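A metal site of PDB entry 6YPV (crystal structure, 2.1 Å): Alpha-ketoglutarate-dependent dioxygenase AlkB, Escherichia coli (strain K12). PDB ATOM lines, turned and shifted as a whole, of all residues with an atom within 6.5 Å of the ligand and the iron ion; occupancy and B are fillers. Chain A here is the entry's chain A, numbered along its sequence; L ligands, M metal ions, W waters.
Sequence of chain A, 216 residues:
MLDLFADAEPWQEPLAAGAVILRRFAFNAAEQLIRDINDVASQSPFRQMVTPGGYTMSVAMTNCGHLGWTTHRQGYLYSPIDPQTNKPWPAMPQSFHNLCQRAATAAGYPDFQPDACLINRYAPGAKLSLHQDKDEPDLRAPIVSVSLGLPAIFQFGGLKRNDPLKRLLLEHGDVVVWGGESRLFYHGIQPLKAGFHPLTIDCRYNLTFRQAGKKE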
ATOM      1  N   MET A  61     -25.559 -18.200   2.816  1.00  0.00           N
ATOM      2  CA  MET A  61     -26.662 -19.150   2.726  1.00  0.00           C
ATOM      3  C   MET A  61     -26.972 -19.506   1.283  1.00  0.00           C
ATOM      4  O   MET A  61     -26.629 -18.787   0.332  1.00  0.00           O
ATOM      5  CB  MET A  61     -27.933 -18.571   3.368  1.00  0.00           C
ATOM      6  CG  MET A  61     -27.884 -18.422   4.871  1.00  0.00           C
ATOM      7  SD  MET A  61     -29.349 -17.582   5.503  1.00  0.00           S
ATOM      8  CE  MET A  61     -29.238 -18.010   7.249  1.00  0.00           C
ATOM      9  N   TRP A  69     -35.617 -20.874   1.719  1.00  0.00           N
ATOM     10  CA  TRP A  69     -35.776 -19.758   2.638  1.00  0.00           C
ATOM     11  C   TRP A  69     -34.953 -18.564   2.165  1.00  0.00           C
ATOM     12  O   TRP A  69     -33.759 -18.690   1.892  1.00  0.00           O
ATOM     13  CB  TRP A  69     -35.354 -20.177   4.037  1.00  0.00           C
ATOM     14  CG  TRP A  69     -35.734 -19.204   5.102  1.00  0.00           C
ATOM     15  CD1 TRP A  69     -36.954 -19.107   5.730  1.00  0.00           C
ATOM     16  CD2 TRP A  69     -34.898 -18.220   5.702  1.00  0.00           C
ATOM     17  NE1 TRP A  69     -36.923 -18.103   6.666  1.00  0.00           N
ATOM     18  CE2 TRP A  69     -35.668 -17.538   6.667  1.00  0.00           C
ATOM     19  CE3 TRP A  69     -33.565 -17.831   5.505  1.00  0.00           C
ATOM     20  CZ2 TRP A  69     -35.150 -16.518   7.447  1.00  0.00           C
ATOM     21  CZ3 TRP A  69     -33.057 -16.802   6.282  1.00  0.00           C
ATOM     22  CH2 TRP A  69     -33.845 -16.153   7.231  1.00  0.00           C
ATOM     23  N   LEU A 118     -32.147 -25.364   4.000  1.00  0.00           N
ATOM     24  CA  LEU A 118     -31.311 -24.177   4.067  1.00  0.00           C
ATOM     25  C   LEU A 118     -29.887 -24.607   4.419  1.00  0.00           C
ATOM     26  O   LEU A 118     -29.679 -25.374   5.369  1.00  0.00           O
ATOM     27  CB  LEU A 118     -31.837 -23.189   5.084  1.00  0.00           C
ATOM     28  CG  LEU A 118     -31.017 -21.918   5.277  1.00  0.00           C
ATOM     29  CD1 LEU A 118     -31.044 -21.040   4.044  1.00  0.00           C
ATOM     30  CD2 LEU A 118     -31.553 -21.143   6.496  1.00  0.00           C
ATOM     31  N   ASN A 120     -26.273 -23.248   5.552  1.00  0.00           N
ATOM     32  CA  ASN A 120     -25.518 -22.153   6.145  1.00  0.00           C
ATOM     33  C   ASN A 120     -24.030 -22.446   6.074  1.00  0.00           C
ATOM     34  O   ASN A 120     -23.606 -23.576   6.326  1.00  0.00           O
ATOM     35  CB  ASN A 120     -25.932 -21.929   7.595  1.00  0.00           C
ATOM     36  CG  ASN A 120     -27.349 -21.413   7.733  1.00  0.00           C
ATOM     37  OD1 ASN A 120     -28.058 -21.230   6.750  1.00  0.00           O
ATOM     38  ND2 ASN A 120     -27.766 -21.165   8.965  1.00  0.00           N
ATOM     39  N   TYR A 122     -20.382 -20.957   7.553  1.00  0.00           N
ATOM     40  CA  TYR A 122     -19.799 -20.093   8.579  1.00  0.00           C
ATOM     41  C   TYR A 122     -18.303 -19.985   8.337  1.00  0.00           C
ATOM     42  O   TYR A 122     -17.583 -20.984   8.463  1.00  0.00           O
ATOM     43  CB  TYR A 122     -20.074 -20.637   9.987  1.00  0.00           C
ATOM     44  CG  TYR A 122     -21.522 -20.661  10.390  1.00  0.00           C
ATOM     45  CD1 TYR A 122     -22.352 -21.711  10.020  1.00  0.00           C
ATOM     46  CD2 TYR A 122     -22.058 -19.643  11.170  1.00  0.00           C
ATOM     47  CE1 TYR A 122     -23.680 -21.741  10.413  1.00  0.00           C
ATOM     48  CE2 TYR A 122     -23.387 -19.667  11.556  1.00  0.00           C
ATOM     49  CZ  TYR A 122     -24.187 -20.712  11.172  1.00  0.00           C
ATOM     50  OH  TYR A 122     -25.519 -20.732  11.575  1.00  0.00           O
ATOM     51  N   LEU A 128     -24.837 -16.398  14.127  1.00  0.00           N
ATOM     52  CA  LEU A 128     -26.272 -16.364  13.838  1.00  0.00           C
ATOM     53  C   LEU A 128     -26.970 -15.921  15.121  1.00  0.00           C
ATOM     54  O   LEU A 128     -26.993 -16.669  16.109  1.00  0.00           O
ATOM     55  CB  LEU A 128     -26.779 -17.724  13.370  1.00  0.00           C
ATOM     56  CG  LEU A 128     -28.199 -17.796  12.821  1.00  0.00           C
ATOM     57  CD1 LEU A 128     -28.397 -16.832  11.654  1.00  0.00           C
ATOM     58  CD2 LEU A 128     -28.535 -19.206  12.405  1.00  0.00           C
ATOM     59  N   HIS A 131     -32.844 -16.309  17.400  1.00  0.00           N
ATOM     60  CA  HIS A 131     -34.013 -16.219  16.536  1.00  0.00           C
ATOM     61  C   HIS A 131     -34.886 -17.423  16.767  1.00  0.00           C
ATOM     62  O   HIS A 131     -34.479 -18.407  17.390  1.00  0.00           O
ATOM     63  CB  HIS A 131     -33.608 -16.126  15.061  1.00  0.00           C
ATOM     64  CG  HIS A 131     -32.953 -17.372  14.546  1.00  0.00           C
ATOM     65  ND1 HIS A 131     -31.626 -17.656  14.761  1.00  0.00           N
ATOM     66  CD2 HIS A 131     -33.451 -18.418  13.850  1.00  0.00           C
ATOM     67  CE1 HIS A 131     -31.328 -18.818  14.213  1.00  0.00           C
ATOM     68  NE2 HIS A 131     -32.421 -19.303  13.647  1.00  0.00           N
ATOM     69  N   GLN A 132     -36.117 -17.345  16.267  1.00  0.00           N
ATOM     70  CA  GLN A 132     -37.031 -18.464  16.207  1.00  0.00           C
ATOM     71  C   GLN A 132     -37.237 -18.874  14.753  1.00  0.00           C
ATOM     72  O   GLN A 132     -37.137 -18.052  13.825  1.00  0.00           O
ATOM     73  CB  GLN A 132     -38.385 -18.115  16.834  1.00  0.00           C
ATOM     74  CG  GLN A 132     -38.421 -18.199  18.348  1.00  0.00           C
ATOM     75  CD  GLN A 132     -39.791 -17.874  18.911  1.00  0.00           C
ATOM     76  OE1 GLN A 132     -40.432 -16.906  18.490  1.00  0.00           O
ATOM     77  NE2 GLN A 132     -40.265 -18.676  19.842  1.00  0.00           N
ATOM     78  N   ASP A 133     -37.531 -20.149  14.548  1.00  0.00           N
ATOM     79  CA  ASP A 133     -37.897 -20.683  13.235  1.00  0.00           C
ATOM     80  C   ASP A 133     -39.395 -20.966  13.278  1.00  0.00           C
ATOM     81  O   ASP A 133     -39.817 -22.066  13.629  1.00  0.00           O
ATOM     82  CB  ASP A 133     -37.085 -21.933  12.904  1.00  0.00           C
ATOM     83  CG  ASP A 133     -35.662 -21.610  12.530  1.00  0.00           C
ATOM     84  OD1 ASP A 133     -35.461 -20.786  11.618  1.00  0.00           O
ATOM     85  OD2 ASP A 133     -34.742 -22.171  13.154  1.00  0.00           O
ATOM     86  N   ILE A 143     -37.592 -29.788  12.734  1.00  0.00           N
ATOM     87  CA  ILE A 143     -36.473 -29.344  11.904  1.00  0.00           C
ATOM     88  C   ILE A 143     -35.294 -30.241  12.217  1.00  0.00           C
ATOM     89  O   ILE A 143     -34.941 -30.442  13.389  1.00  0.00           O
ATOM     90  CB  ILE A 143     -36.122 -27.866  12.159  1.00  0.00           C
ATOM     91  CG1 ILE A 143     -37.161 -26.957  11.501  1.00  0.00           C
ATOM     92  CG2 ILE A 143     -34.721 -27.554  11.624  1.00  0.00           C
ATOM     93  CD1 ILE A 143     -36.989 -25.490  11.800  1.00  0.00           C
ATOM     94  N   SER A 145     -31.335 -30.768  11.859  1.00  0.00           N
ATOM     95  CA  SER A 145     -30.142 -29.935  11.710  1.00  0.00           C
ATOM     96  C   SER A 145     -28.905 -30.823  11.628  1.00  0.00           C
ATOM     97  O   SER A 145     -28.716 -31.715  12.458  1.00  0.00           O
ATOM     98  CB  SER A 145     -30.021 -28.955  12.877  1.00  0.00           C
ATOM     99  OG  SER A 145     -28.868 -28.162  12.721  1.00  0.00           O
ATOM    100  N   VAL A 146     -28.073 -30.551  10.631  1.00  0.00           N
ATOM    101  CA  VAL A 146     -26.860 -31.324  10.369  1.00  0.00           C
ATOM    102  C   VAL A 146     -25.671 -30.373  10.421  1.00  0.00           C
ATOM    103  O   VAL A 146     -25.653 -29.373   9.708  1.00  0.00           O
ATOM    104  CB  VAL A 146     -26.920 -32.040   9.002  1.00  0.00           C
ATOM    105  CG1 VAL A 146     -25.636 -32.839   8.761  1.00  0.00           C
ATOM    106  CG2 VAL A 146     -28.153 -32.929   8.934  1.00  0.00           C
ATOM    107  N   SER A 147     -24.683 -30.704  11.245  1.00  0.00           N
ATOM    108  CA  SER A 147     -23.485 -29.891  11.412  1.00  0.00           C
ATOM    109  C   SER A 147     -22.295 -30.567  10.743  1.00  0.00           C
ATOM    110  O   SER A 147     -22.087 -31.779  10.891  1.00  0.00           O
ATOM    111  CB  SER A 147     -23.174 -29.663  12.898  1.00  0.00           C
ATOM    112  OG  SER A 147     -24.072 -28.747  13.478  1.00  0.00           O
ATOM    113  N   ALA A 152     -18.968 -25.577  16.583  1.00  0.00           N
ATOM    114  CA  ALA A 152     -19.662 -24.335  16.875  1.00  0.00           C
ATOM    115  C   ALA A 152     -20.361 -24.432  18.221  1.00  0.00           C
ATOM    116  O   ALA A 152     -20.765 -25.521  18.650  1.00  0.00           O
ATOM    117  CB  ALA A 152     -20.694 -24.005  15.789  1.00  0.00           C
ATOM    118  N   PHE A 154     -23.541 -23.790  19.912  1.00  0.00           N
ATOM    119  CA  PHE A 154     -24.966 -23.586  19.718  1.00  0.00           C
ATOM    120  C   PHE A 154     -25.586 -23.176  21.042  1.00  0.00           C
ATOM    121  O   PHE A 154     -25.364 -23.812  22.075  1.00  0.00           O
ATOM    122  CB  PHE A 154     -25.617 -24.874  19.187  1.00  0.00           C
ATOM    123  CG  PHE A 154     -27.094 -24.764  18.950  1.00  0.00           C
ATOM    124  CD1 PHE A 154     -27.585 -24.236  17.767  1.00  0.00           C
ATOM    125  CD2 PHE A 154     -27.992 -25.207  19.903  1.00  0.00           C
ATOM    126  CE1 PHE A 154     -28.947 -24.150  17.547  1.00  0.00           C
ATOM    127  CE2 PHE A 154     -29.348 -25.114  19.688  1.00  0.00           C
ATOM    128  CZ  PHE A 154     -29.822 -24.592  18.497  1.00  0.00           C
ATOM    129  N   LEU A 170     -21.613 -28.148  19.061  1.00  0.00           N
ATOM    130  CA  LEU A 170     -22.005 -28.988  17.931  1.00  0.00           C
ATOM    131  C   LEU A 170     -20.772 -29.224  17.067  1.00  0.00           C
ATOM    132  O   LEU A 170     -20.117 -28.267  16.626  1.00  0.00           O
ATOM    133  CB  LEU A 170     -23.112 -28.334  17.117  1.00  0.00           C
ATOM    134  CG  LEU A 170     -24.490 -28.264  17.770  1.00  0.00           C
ATOM    135  CD1 LEU A 170     -25.487 -27.569  16.867  1.00  0.00           C
ATOM    136  CD2 LEU A 170     -24.989 -29.657  18.141  1.00  0.00           C
ATOM    137  N   HIS A 187     -32.797 -19.610  19.481  1.00  0.00           N
ATOM    138  CA  HIS A 187     -31.512 -20.289  19.329  1.00  0.00           C
ATOM    139  C   HIS A 187     -30.623 -19.471  18.407  1.00  0.00           C
ATOM    140  O   HIS A 187     -31.097 -18.583  17.687  1.00  0.00           O
ATOM    141  CB  HIS A 187     -31.683 -21.709  18.781  1.00  0.00           C
ATOM    142  CG  HIS A 187     -32.403 -21.750  17.469  1.00  0.00           C
ATOM    143  ND1 HIS A 187     -33.779 -21.796  17.360  1.00  0.00           N
ATOM    144  CD2 HIS A 187     -31.927 -21.760  16.192  1.00  0.00           C
ATOM    145  CE1 HIS A 187     -34.121 -21.837  16.090  1.00  0.00           C
ATOM    146  NE2 HIS A 187     -33.030 -21.819  15.355  1.00  0.00           N
ATOM    147  N   GLY A 188     -29.330 -19.795  18.434  1.00  0.00           N
ATOM    148  CA  GLY A 188     -28.372 -19.082  17.610  1.00  0.00           C
ATOM    149  C   GLY A 188     -27.015 -19.750  17.698  1.00  0.00           C
ATOM    150  O   GLY A 188     -26.844 -20.791  18.328  1.00  0.00           O
ATOM    151  N   ILE A 189     -26.040 -19.122  17.043  1.00  0.00           N
ATOM    152  CA  ILE A 189     -24.677 -19.636  16.984  1.00  0.00           C
ATOM    153  C   ILE A 189     -23.736 -18.513  17.367  1.00  0.00           C
ATOM    154  O   ILE A 189     -23.844 -17.398  16.841  1.00  0.00           O
ATOM    155  CB  ILE A 189     -24.333 -20.168  15.582  1.00  0.00           C
ATOM    156  CG1 ILE A 189     -25.173 -21.418  15.257  1.00  0.00           C
ATOM    157  CG2 ILE A 189     -22.857 -20.484  15.476  1.00  0.00           C
ATOM    158  CD1 ILE A 189     -24.769 -22.637  16.016  1.00  0.00           C
ATOM    159  N   ARG A 204     -17.612 -23.945   8.692  1.00  0.00           N
ATOM    160  CA  ARG A 204     -18.634 -24.868   9.165  1.00  0.00           C
ATOM    161  C   ARG A 204     -19.845 -24.764   8.250  1.00  0.00           C
ATOM    162  O   ARG A 204     -20.244 -23.663   7.853  1.00  0.00           O
ATOM    163  CB  ARG A 204     -19.033 -24.559  10.610  1.00  0.00           C
ATOM    164  CG  ARG A 204     -20.285 -25.289  11.095  1.00  0.00           C
ATOM    165  CD  ARG A 204     -20.658 -24.908  12.521  1.00  0.00           C
ATOM    166  NE  ARG A 204     -21.807 -25.649  13.036  1.00  0.00           N
ATOM    167  CZ  ARG A 204     -23.058 -25.184  13.072  1.00  0.00           C
ATOM    168  NH1 ARG A 204     -23.346 -23.970  12.657  1.00  0.00           N
ATOM    169  NH2 ARG A 204     -24.035 -25.949  13.552  1.00  0.00           N
ATOM    170  N   TYR A 205     -20.416 -25.914   7.912  1.00  0.00           N
ATOM    171  CA  TYR A 205     -21.689 -25.971   7.201  1.00  0.00           C
ATOM    172  C   TYR A 205     -22.779 -26.485   8.140  1.00  0.00           C
ATOM    173  O   TYR A 205     -22.536 -27.362   8.976  1.00  0.00           O
ATOM    174  CB  TYR A 205     -21.617 -26.880   5.977  1.00  0.00           C
ATOM    175  CG  TYR A 205     -20.670 -26.404   4.909  1.00  0.00           C
ATOM    176  CD1 TYR A 205     -21.016 -25.382   4.047  1.00  0.00           C
ATOM    177  CD2 TYR A 205     -19.419 -27.008   4.752  1.00  0.00           C
ATOM    178  CE1 TYR A 205     -20.148 -24.949   3.062  1.00  0.00           C
ATOM    179  CE2 TYR A 205     -18.544 -26.571   3.755  1.00  0.00           C
ATOM    180  CZ  TYR A 205     -18.927 -25.557   2.918  1.00  0.00           C
ATOM    181  OH  TYR A 205     -18.060 -25.124   1.933  1.00  0.00           O
ATOM    182  N   ASN A 206     -23.968 -25.930   8.001  1.00  0.00           N
ATOM    183  CA  ASN A 206     -25.144 -26.414   8.716  1.00  0.00           C
ATOM    184  C   ASN A 206     -26.292 -26.565   7.725  1.00  0.00           C
ATOM    185  O   ASN A 206     -26.562 -25.644   6.949  1.00  0.00           O
ATOM    186  CB  ASN A 206     -25.539 -25.467   9.842  1.00  0.00           C
ATOM    187  CG  ASN A 206     -26.740 -25.960  10.607  1.00  0.00           C
ATOM    188  OD1 ASN A 206     -27.869 -25.522  10.359  1.00  0.00           O
ATOM    189  ND2 ASN A 206     -26.516 -26.866  11.545  1.00  0.00           N
ATOM    190  N   THR A 208     -30.395 -27.328   7.573  1.00  0.00           N
ATOM    191  CA  THR A 208     -31.648 -27.408   8.327  1.00  0.00           C
ATOM    192  C   THR A 208     -32.751 -27.850   7.369  1.00  0.00           C
ATOM    193  O   THR A 208     -33.141 -27.091   6.481  1.00  0.00           O
ATOM    194  CB  THR A 208     -31.997 -26.079   8.991  1.00  0.00           C
ATOM    195  OG1 THR A 208     -31.722 -24.994   8.099  1.00  0.00           O
ATOM    196  CG2 THR A 208     -31.187 -25.891  10.265  1.00  0.00           C
ATOM    197  N   ARG A 210     -36.518 -28.672   6.434  1.00  0.00           N
ATOM    198  CA  ARG A 210     -37.777 -28.063   6.837  1.00  0.00           C
ATOM    199  C   ARG A 210     -38.933 -28.574   5.988  1.00  0.00           C
ATOM    200  O   ARG A 210     -38.774 -28.868   4.804  1.00  0.00           O
ATOM    201  CB  ARG A 210     -37.722 -26.531   6.724  1.00  0.00           C
ATOM    202  CG  ARG A 210     -36.627 -25.893   7.552  1.00  0.00           C
ATOM    203  CD  ARG A 210     -35.764 -24.963   6.716  1.00  0.00           C
ATOM    204  NE  ARG A 210     -34.675 -24.402   7.512  1.00  0.00           N
ATOM    205  CZ  ARG A 210     -34.821 -23.378   8.353  1.00  0.00           C
ATOM    206  NH1 ARG A 210     -36.004 -22.802   8.501  1.00  0.00           N
ATOM    207  NH2 ARG A 210     -33.772 -22.943   9.032  1.00  0.00           N
HETATM  208  C1  LIG L   1     -30.988 -21.612  11.019  1.00  0.00           C
HETATM  209  O1  LIG L   1     -30.418 -21.446   9.914  1.00  0.00           O
HETATM  210  O2  LIG L   1     -32.233 -21.420  11.138  1.00  0.00           O
HETATM  211  C2  LIG L   1     -30.171 -22.052  12.240  1.00  0.00           C
HETATM  212  O3  LIG L   1     -30.615 -21.915  13.326  1.00  0.00           O
HETATM  213  C3  LIG L   1     -28.782 -22.655  12.034  1.00  0.00           C
HETATM  214  C4  LIG L   1     -28.268 -23.173  13.379  1.00  0.00           C
HETATM  215  C5  LIG L   1     -26.857 -23.723  13.180  1.00  0.00           C
HETATM  216  O4  LIG L   1     -26.067 -23.144  12.391  1.00  0.00           O
HETATM  217  O5  LIG L   1     -26.494 -24.761  13.799  1.00  0.00           O
HETATM  218 FE    FE M   1     -32.863 -21.589  13.261  1.00  0.00          FE
HETATM  219  O   HOH W   1     -28.247 -26.720  14.731  1.00  0.00           O
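Water W1 bridges the side-chain hydroxyl (OG) of Ser 145 (2.6 Å) and an oxygen (O5) of the ligand (2.8 Å).
Leu 118 touches the ligand.
CD2 of Leu 128 touches C2 of the ligand, 3.3 Å away.
Ile 189 touches the ligand.
Hydrophobic or aromatic side chains that line the ligand: Leu 118, Tyr 122, Leu 128, His 131, His 187 and Ile 189.
11 residues have an atom within 4 Å of the ligand: Leu 118, Asn 120, Tyr 122, Leu 128, His 131, Asp 133, His 187, Ile 189, Arg 204, Asn 206 and Arg 210.
The nearest printed residue that does not touch the ligand is Phe 154 (4.1 Å).
OD2 of Asp 133 binds the iron ion, 2.0 Å away.
A ring nitrogen (NE2) of His 187 is bound to the iron ion.
An oxygen (O2) of the ligand is bound to the iron ion, at 2.2 Å.
The iron ion is bound by O3 of the ligand, 2.3 Å away.
NE2 of His 131 binds the iron ion, 2.4 Å away.
An oxygen (O4) of the ligand sits at hydrogen-bond distance from the side-chain hydroxyl (OH) of Tyr 122.
The guanidinium group of Arg 204 is in salt-bridge range of an oxygen (O5) of the ligand, at 2.7 Å.
ND2 of Asn 120 is in hydrogen-bond range of O1 of the ligand, 2.8 Å away.
NH2 of Arg 210 is in salt-bridge range of O1 of the ligand (3.8 Å).
The side-chain amide nitrogen (ND2) of Asn 206 lies within hydrogen-bond range of an oxygen (O5) of the ligand, 3.1 Å away.
Of the 24 residues printed, 3 come within 4 Å of the iron ion.
The nearest printed residue that does not touch the iron ion is Arg 210 (4.5 Å).
OH of Tyr 122 is in hydrogen-bond range of ND2 of Asn 120, 3.5 Å away.
The side-chain amide nitrogen (ND2) of Asn 206 lies close to the guanidinium group (NH2) of Arg 204.
The guanidinium group (NH2) of Arg 204 sits at hydrogen-bond distance from the side-chain hydroxyl (OG) of Ser 147.
O of Asn 206 sits at hydrogen-bond distance from N of Asn 120, at 2.8 Å.
OG1 of Thr 208 sits at hydrogen-bond distance from NH2 of Arg 210 (3.0 Å).
ND2 of Asn 206 sits at hydrogen-bond distance from OG of Ser 145, at 2.9 Å.
N of Ile 189 sits at hydrogen-bond distance from O of Leu 128, 2.8 Å away.
The backbone carbonyl oxygen (O) of Leu 118 sits at hydrogen-bond distance from the backbone NH (N) of Thr 208 (3.0 Å).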
